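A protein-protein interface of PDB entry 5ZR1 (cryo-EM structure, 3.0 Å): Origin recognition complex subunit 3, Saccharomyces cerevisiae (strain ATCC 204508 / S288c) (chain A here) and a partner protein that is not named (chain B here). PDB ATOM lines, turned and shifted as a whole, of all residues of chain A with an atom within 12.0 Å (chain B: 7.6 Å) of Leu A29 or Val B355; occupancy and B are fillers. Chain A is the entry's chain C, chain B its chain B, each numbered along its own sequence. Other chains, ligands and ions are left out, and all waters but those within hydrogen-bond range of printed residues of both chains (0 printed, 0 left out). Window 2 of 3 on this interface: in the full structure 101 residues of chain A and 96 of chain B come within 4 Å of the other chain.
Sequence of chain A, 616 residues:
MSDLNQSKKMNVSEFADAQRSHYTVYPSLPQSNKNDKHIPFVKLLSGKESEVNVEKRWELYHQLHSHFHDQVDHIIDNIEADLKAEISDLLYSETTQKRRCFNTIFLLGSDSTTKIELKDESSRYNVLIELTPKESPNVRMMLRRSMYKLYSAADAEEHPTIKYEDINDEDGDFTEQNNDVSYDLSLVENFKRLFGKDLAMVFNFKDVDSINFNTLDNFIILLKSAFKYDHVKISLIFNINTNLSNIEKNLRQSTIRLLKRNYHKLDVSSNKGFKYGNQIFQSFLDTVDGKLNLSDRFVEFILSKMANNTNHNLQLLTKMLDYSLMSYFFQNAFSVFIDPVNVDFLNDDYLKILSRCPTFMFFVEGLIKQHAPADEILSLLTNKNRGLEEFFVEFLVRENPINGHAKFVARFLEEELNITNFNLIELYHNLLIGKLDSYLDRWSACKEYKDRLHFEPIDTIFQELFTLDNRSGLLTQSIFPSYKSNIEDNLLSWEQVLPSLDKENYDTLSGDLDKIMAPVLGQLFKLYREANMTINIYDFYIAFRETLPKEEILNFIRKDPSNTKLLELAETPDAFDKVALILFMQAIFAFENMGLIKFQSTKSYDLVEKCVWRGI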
ATOM      1  N   VAL A  25     -21.196  -4.073  -7.096  1.00  0.00           N
ATOM      2  CA  VAL A  25     -21.274  -4.125  -5.644  1.00  0.00           C
ATOM      3  C   VAL A  25     -21.697  -5.530  -5.250  1.00  0.00           C
ATOM      4  O   VAL A  25     -22.642  -6.083  -5.822  1.00  0.00           O
ATOM      5  CB  VAL A  25     -22.259  -3.076  -5.103  1.00  0.00           C
ATOM      6  CG1 VAL A  25     -22.433  -3.209  -3.602  1.00  0.00           C
ATOM      7  CG2 VAL A  25     -21.779  -1.692  -5.447  1.00  0.00           C
ATOM      8  N   TYR A  26     -20.968  -6.124  -4.315  1.00  0.00           N
ATOM      9  CA  TYR A  26     -21.409  -7.316  -3.612  1.00  0.00           C
ATOM     10  C   TYR A  26     -21.860  -6.856  -2.233  1.00  0.00           C
ATOM     11  O   TYR A  26     -21.046  -6.815  -1.303  1.00  0.00           O
ATOM     12  CB  TYR A  26     -20.283  -8.342  -3.512  1.00  0.00           C
ATOM     13  CG  TYR A  26     -19.885  -8.976  -4.826  1.00  0.00           C
ATOM     14  CD1 TYR A  26     -20.761  -9.014  -5.899  1.00  0.00           C
ATOM     15  CD2 TYR A  26     -18.616  -9.505  -4.999  1.00  0.00           C
ATOM     16  CE1 TYR A  26     -20.390  -9.587  -7.097  1.00  0.00           C
ATOM     17  CE2 TYR A  26     -18.237 -10.076  -6.199  1.00  0.00           C
ATOM     18  CZ  TYR A  26     -19.131 -10.111  -7.244  1.00  0.00           C
ATOM     19  OH  TYR A  26     -18.768 -10.677  -8.443  1.00  0.00           O
ATOM     20  N   PRO A  27     -23.124  -6.483  -2.064  1.00  0.00           N
ATOM     21  CA  PRO A  27     -23.533  -5.779  -0.847  1.00  0.00           C
ATOM     22  C   PRO A  27     -23.628  -6.703   0.356  1.00  0.00           C
ATOM     23  O   PRO A  27     -23.834  -7.913   0.244  1.00  0.00           O
ATOM     24  CB  PRO A  27     -24.906  -5.210  -1.215  1.00  0.00           C
ATOM     25  CG  PRO A  27     -25.417  -6.136  -2.234  1.00  0.00           C
ATOM     26  CD  PRO A  27     -24.239  -6.619  -3.015  1.00  0.00           C
ATOM     27  N   SER A  28     -23.459  -6.096   1.526  1.00  0.00           N
ATOM     28  CA  SER A  28     -23.443  -6.815   2.788  1.00  0.00           C
ATOM     29  C   SER A  28     -24.865  -7.003   3.293  1.00  0.00           C
ATOM     30  O   SER A  28     -25.619  -6.034   3.426  1.00  0.00           O
ATOM     31  CB  SER A  28     -22.611  -6.060   3.822  1.00  0.00           C
ATOM     32  OG  SER A  28     -23.220  -4.824   4.149  1.00  0.00           O
ATOM     33  N   LEU A  29     -25.223  -8.245   3.572  1.00  0.00           N
ATOM     34  CA  LEU A  29     -26.545  -8.508   4.114  1.00  0.00           C
ATOM     35  C   LEU A  29     -26.467  -8.669   5.626  1.00  0.00           C
ATOM     36  O   LEU A  29     -25.499  -9.245   6.138  1.00  0.00           O
ATOM     37  CB  LEU A  29     -27.156  -9.764   3.479  1.00  0.00           C
ATOM     38  CG  LEU A  29     -26.742 -11.208   3.794  1.00  0.00           C
ATOM     39  CD1 LEU A  29     -27.756 -12.164   3.200  1.00  0.00           C
ATOM     40  CD2 LEU A  29     -25.348 -11.560   3.296  1.00  0.00           C
ATOM     41  N   PRO A  30     -27.445  -8.141   6.376  1.00  0.00           N
ATOM     42  CA  PRO A  30     -27.415  -8.287   7.840  1.00  0.00           C
ATOM     43  C   PRO A  30     -27.657  -9.717   8.304  1.00  0.00           C
ATOM     44  O   PRO A  30     -27.933 -10.603   7.489  1.00  0.00           O
ATOM     45  CB  PRO A  30     -28.523  -7.338   8.312  1.00  0.00           C
ATOM     46  CG  PRO A  30     -29.431  -7.201   7.141  1.00  0.00           C
ATOM     47  CD  PRO A  30     -28.554  -7.280   5.929  1.00  0.00           C
ATOM     48  N   GLN A  31     -27.571  -9.937   9.619  1.00  0.00           N
ATOM     49  CA  GLN A  31     -27.386 -11.286  10.151  1.00  0.00           C
ATOM     50  C   GLN A  31     -28.655 -12.135  10.005  1.00  0.00           C
ATOM     51  O   GLN A  31     -28.621 -13.210   9.397  1.00  0.00           O
ATOM     52  CB  GLN A  31     -26.865 -11.195  11.606  1.00  0.00           C
ATOM     53  CG  GLN A  31     -27.747 -10.534  12.698  1.00  0.00           C
ATOM     54  CD  GLN A  31     -27.729  -9.011  12.682  1.00  0.00           C
ATOM     55  OE1 GLN A  31     -27.276  -8.386  11.724  1.00  0.00           O
ATOM     56  NE2 GLN A  31     -28.260  -8.409  13.739  1.00  0.00           N
ATOM     57  N   SER A  32     -29.786 -11.643  10.520  1.00  0.00           N
ATOM     58  CA  SER A  32     -31.129 -12.191  10.369  1.00  0.00           C
ATOM     59  C   SER A  32     -32.072 -11.144  10.938  1.00  0.00           C
ATOM     60  O   SER A  32     -31.853 -10.670  12.056  1.00  0.00           O
ATOM     61  CB  SER A  32     -31.297 -13.529  11.102  1.00  0.00           C
ATOM     62  OG  SER A  32     -32.614 -14.034  10.958  1.00  0.00           O
ATOM     63  N   ASN A  33     -33.119 -10.764  10.206  1.00  0.00           N
ATOM     64  CA  ASN A  33     -34.016  -9.732  10.714  1.00  0.00           C
ATOM     65  C   ASN A  33     -35.216 -10.312  11.450  1.00  0.00           C
ATOM     66  O   ASN A  33     -36.312  -9.734  11.397  1.00  0.00           O
ATOM     67  CB  ASN A  33     -34.468  -8.795   9.594  1.00  0.00           C
ATOM     68  CG  ASN A  33     -33.311  -8.046   8.966  1.00  0.00           C
ATOM     69  OD1 ASN A  33     -32.228  -7.990   9.520  1.00  0.00           O
ATOM     70  ND2 ASN A  33     -33.578  -7.361   7.882  1.00  0.00           N
ATOM     71  N   LYS A  34     -35.035 -11.469  12.094  1.00  0.00           N
ATOM     72  CA  LYS A  34     -35.885 -12.056  13.132  1.00  0.00           C
ATOM     73  C   LYS A  34     -37.241 -12.512  12.616  1.00  0.00           C
ATOM     74  O   LYS A  34     -38.098 -12.904  13.418  1.00  0.00           O
ATOM     75  CB  LYS A  34     -36.120 -11.102  14.314  1.00  0.00           C
ATOM     76  CG  LYS A  34     -34.930 -10.864  15.249  1.00  0.00           C
ATOM     77  CD  LYS A  34     -34.004  -9.775  14.712  1.00  0.00           C
ATOM     78  CE  LYS A  34     -32.880  -9.452  15.666  1.00  0.00           C
ATOM     79  NZ  LYS A  34     -31.933  -8.485  15.045  1.00  0.00           N
ATOM     80  N   ASN A  35     -37.466 -12.485  11.305  1.00  0.00           N
ATOM     81  CA  ASN A  35     -38.820 -12.553  10.780  1.00  0.00           C
ATOM     82  C   ASN A  35     -38.842 -13.297   9.456  1.00  0.00           C
ATOM     83  O   ASN A  35     -37.862 -13.304   8.707  1.00  0.00           O
ATOM     84  CB  ASN A  35     -39.401 -11.148  10.588  1.00  0.00           C
ATOM     85  CG  ASN A  35     -39.773 -10.481  11.896  1.00  0.00           C
ATOM     86  OD1 ASN A  35     -40.345 -11.111  12.785  1.00  0.00           O
ATOM     87  ND2 ASN A  35     -39.448  -9.200  12.022  1.00  0.00           N
ATOM     88  N   HIS A  38     -40.654 -11.519   4.628  1.00  0.00           N
ATOM     89  CA  HIS A  38     -40.027 -11.084   3.382  1.00  0.00           C
ATOM     90  C   HIS A  38     -40.969 -11.280   2.193  1.00  0.00           C
ATOM     91  O   HIS A  38     -40.721 -12.059   1.275  1.00  0.00           O
ATOM     92  CB  HIS A  38     -38.706 -11.807   3.170  1.00  0.00           C
ATOM     93  CG  HIS A  38     -37.724 -11.588   4.274  1.00  0.00           C
ATOM     94  ND1 HIS A  38     -37.484 -12.530   5.252  1.00  0.00           N
ATOM     95  CD2 HIS A  38     -36.976 -10.508   4.601  1.00  0.00           C
ATOM     96  CE1 HIS A  38     -36.590 -12.058   6.102  1.00  0.00           C
ATOM     97  NE2 HIS A  38     -36.267 -10.833   5.732  1.00  0.00           N
ATOM     98  N   ILE B 331     -29.145  -1.091  -3.435  1.00  0.00           N
ATOM     99  CA  ILE B 331     -28.145  -1.758  -2.609  1.00  0.00           C
ATOM    100  C   ILE B 331     -28.651  -1.981  -1.192  1.00  0.00           C
ATOM    101  O   ILE B 331     -28.584  -3.096  -0.669  1.00  0.00           O
ATOM    102  CB  ILE B 331     -26.825  -0.961  -2.621  1.00  0.00           C
ATOM    103  CG1 ILE B 331     -26.236  -0.943  -4.030  1.00  0.00           C
ATOM    104  CG2 ILE B 331     -25.835  -1.548  -1.639  1.00  0.00           C
ATOM    105  CD1 ILE B 331     -25.076   0.000  -4.187  1.00  0.00           C
ATOM    106  N   SER B 335     -31.486  -5.452  -2.660  1.00  0.00           N
ATOM    107  CA  SER B 335     -30.618  -6.624  -2.715  1.00  0.00           C
ATOM    108  C   SER B 335     -30.634  -7.520  -1.470  1.00  0.00           C
ATOM    109  O   SER B 335     -30.581  -8.743  -1.640  1.00  0.00           O
ATOM    110  CB  SER B 335     -29.186  -6.191  -3.038  1.00  0.00           C
ATOM    111  OG  SER B 335     -28.335  -7.316  -3.102  1.00  0.00           O
ATOM    112  N   PRO B 336     -30.694  -7.017  -0.220  1.00  0.00           N
ATOM    113  CA  PRO B 336     -30.876  -7.961   0.892  1.00  0.00           C
ATOM    114  C   PRO B 336     -32.254  -8.582   0.946  1.00  0.00           C
ATOM    115  O   PRO B 336     -32.393  -9.696   1.464  1.00  0.00           O
ATOM    116  CB  PRO B 336     -30.613  -7.106   2.136  1.00  0.00           C
ATOM    117  CG  PRO B 336     -29.815  -6.007   1.674  1.00  0.00           C
ATOM    118  CD  PRO B 336     -30.323  -5.694   0.322  1.00  0.00           C
ATOM    119  N   LYS B 337     -33.278  -7.911   0.435  1.00  0.00           N
ATOM    120  CA  LYS B 337     -34.630  -8.402   0.633  1.00  0.00           C
ATOM    121  C   LYS B 337     -35.097  -9.342  -0.461  1.00  0.00           C
ATOM    122  O   LYS B 337     -36.053 -10.090  -0.242  1.00  0.00           O
ATOM    123  CB  LYS B 337     -35.600  -7.230   0.778  1.00  0.00           C
ATOM    124  CG  LYS B 337     -35.361  -6.484   2.074  1.00  0.00           C
ATOM    125  CD  LYS B 337     -36.342  -5.378   2.291  1.00  0.00           C
ATOM    126  CE  LYS B 337     -37.695  -5.930   2.679  1.00  0.00           C
ATOM    127  NZ  LYS B 337     -37.650  -6.543   4.030  1.00  0.00           N
ATOM    128  N   ALA B 339     -32.807 -11.573  -1.520  1.00  0.00           N
ATOM    129  CA  ALA B 339     -32.037 -12.735  -1.076  1.00  0.00           C
ATOM    130  C   ALA B 339     -32.703 -13.442   0.095  1.00  0.00           C
ATOM    131  O   ALA B 339     -32.665 -14.674   0.186  1.00  0.00           O
ATOM    132  CB  ALA B 339     -30.622 -12.310  -0.694  1.00  0.00           C
ATOM    133  N   TYR B 340     -33.309 -12.682   1.004  1.00  0.00           N
ATOM    134  CA  TYR B 340     -34.056 -13.294   2.092  1.00  0.00           C
ATOM    135  C   TYR B 340     -35.341 -13.939   1.596  1.00  0.00           C
ATOM    136  O   TYR B 340     -35.790 -14.939   2.165  1.00  0.00           O
ATOM    137  CB  TYR B 340     -34.373 -12.247   3.152  1.00  0.00           C
ATOM    138  CG  TYR B 340     -33.188 -11.776   3.949  1.00  0.00           C
ATOM    139  CD1 TYR B 340     -32.055 -12.563   4.078  1.00  0.00           C
ATOM    140  CD2 TYR B 340     -33.190 -10.521   4.545  1.00  0.00           C
ATOM    141  CE1 TYR B 340     -30.970 -12.128   4.804  1.00  0.00           C
ATOM    142  CE2 TYR B 340     -32.106 -10.073   5.268  1.00  0.00           C
ATOM    143  CZ  TYR B 340     -30.998 -10.882   5.392  1.00  0.00           C
ATOM    144  OH  TYR B 340     -29.912 -10.446   6.112  1.00  0.00           O
ATOM    145  N   LEU B 343     -35.090 -17.722   0.205  1.00  0.00           N
ATOM    146  CA  LEU B 343     -34.754 -18.821   1.096  1.00  0.00           C
ATOM    147  C   LEU B 343     -36.019 -19.493   1.612  1.00  0.00           C
ATOM    148  O   LEU B 343     -36.326 -20.625   1.243  1.00  0.00           O
ATOM    149  CB  LEU B 343     -33.902 -18.334   2.265  1.00  0.00           C
ATOM    150  CG  LEU B 343     -32.504 -17.829   1.908  1.00  0.00           C
ATOM    151  CD1 LEU B 343     -31.792 -17.311   3.145  1.00  0.00           C
ATOM    152  CD2 LEU B 343     -31.699 -18.928   1.239  1.00  0.00           C
ATOM    153  N   VAL B 355     -24.913 -17.859   2.930  1.00  0.00           N
ATOM    154  CA  VAL B 355     -25.838 -16.997   2.208  1.00  0.00           C
ATOM    155  C   VAL B 355     -25.104 -15.711   1.818  1.00  0.00           C
ATOM    156  O   VAL B 355     -24.198 -15.260   2.522  1.00  0.00           O
ATOM    157  CB  VAL B 355     -27.128 -16.735   3.053  1.00  0.00           C
ATOM    158  CG1 VAL B 355     -26.830 -15.923   4.313  1.00  0.00           C
ATOM    159  CG2 VAL B 355     -28.239 -16.093   2.219  1.00  0.00           C
ATOM    160  N   ASN B 356     -25.457 -15.154   0.661  1.00  0.00           N
ATOM    161  CA  ASN B 356     -24.861 -13.916   0.189  1.00  0.00           C
ATOM    162  C   ASN B 356     -25.916 -13.161  -0.608  1.00  0.00           C
ATOM    163  O   ASN B 356     -26.889 -13.746  -1.090  1.00  0.00           O
ATOM    164  CB  ASN B 356     -23.604 -14.188  -0.652  1.00  0.00           C
ATOM    165  CG  ASN B 356     -22.728 -12.958  -0.820  1.00  0.00           C
ATOM    166  OD1 ASN B 356     -23.061 -11.872  -0.346  1.00  0.00           O
ATOM    167  ND2 ASN B 356     -21.593 -13.130  -1.486  1.00  0.00           N
ATOM    168  N   SER B 357     -25.720 -11.851  -0.733  1.00  0.00           N
ATOM    169  CA  SER B 357     -26.680 -11.013  -1.429  1.00  0.00           C
ATOM    170  C   SER B 357     -26.586 -11.207  -2.939  1.00  0.00           C
ATOM    171  O   SER B 357     -25.672 -11.848  -3.464  1.00  0.00           O
ATOM    172  CB  SER B 357     -26.462  -9.542  -1.092  1.00  0.00           C
ATOM    173  OG  SER B 357     -26.732  -9.280   0.268  1.00  0.00           O
ATOM    174  N   ILE B 358     -27.553 -10.631  -3.637  1.00  0.00           N
ATOM    175  CA  ILE B 358     -27.532 -10.602  -5.102  1.00  0.00           C
ATOM    176  C   ILE B 358     -26.480  -9.598  -5.556  1.00  0.00           C
ATOM    177  O   ILE B 358     -26.414  -8.487  -5.002  1.00  0.00           O
ATOM    178  CB  ILE B 358     -28.922 -10.241  -5.648  1.00  0.00           C
ATOM    179  CG1 ILE B 358     -29.908 -11.387  -5.442  1.00  0.00           C
ATOM    180  CG2 ILE B 358     -28.885  -9.866  -7.109  1.00  0.00           C
ATOM    181  CD1 ILE B 358     -30.753 -11.244  -4.243  1.00  0.00           C
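O of Pro A27 lies within hydrogen-bond range of OG of Ser B357 (3.2 Å).
OH of Tyr B340 is in hydrogen-bond range of O of Pro A30, 2.4 Å away.
The side-chain hydroxyl of Ser B335 lies within hydrogen-bond range of the backbone carbonyl oxygen of Ile B358.
Among the printed residues, pairs that only touch across the chains: Val A25 with Ile B331 (3.9 Å), Pro A27 with Ile B331 (3.8 Å), Pro A27 with Ser B335 (3.3 Å), Pro A27 with Ile B358 (3.5 Å), Leu A29 with Tyr B340 (3.6 Å), Leu A29 with Val B355 (3.95 Å), Leu A29 with Asn B356 (3.9 Å), Leu A29 with Ser B357 (3.3 Å) and His A38 with Tyr B340 (3.3 Å).
Leu A29 touches just these residues of chain B: Tyr B340 (3.6 Å), Val B355 (3.95 Å), Asn B356 (3.9 Å) and Ser B357 (3.3 Å).
Of chain A, only Leu A29 (3.95 Å) comes within 4 Å of Val B355.
No residue of chain A comes within 4 Å of Pro B336.
Of the printed residues of chain A, Ile B331 touches Val A25 and Pro A27.
Of the printed residues of chain A, Ser B335 touches Pro A27.
Of the printed residues of chain B, Val A25 touches Ile B331.
Printed residues of chain B within 4 Å of His A38: Tyr B340 (3.3 Å).
Of the printed residues of chain B, Pro A30 touches Tyr B340 (2.4 Å).
Gln A31 touches none of the printed residues of chain B.
Asn A35 touches none of the printed residues of chain B.
The nearest residue of chain A that does not touch Val B355 is Gln A31 (6.0 Å).
Of the 11 printed residues of chain B, 7 touch a printed residue of chain A.
Hydrophobic or aromatic side chains of chain B that line the printed part of chain A: Ile B331 and Tyr B340.
Along chain B the printed residues that touch a printed residue of chain A span positions 331 to 358.
Hydrophobic or aromatic side chains of chain A within 4 Å of the printed part of chain B: Val A25, Pro A27, Leu A29, Pro A30 and His A38.
Among the printed residues, 11 pairs touch across the chains.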
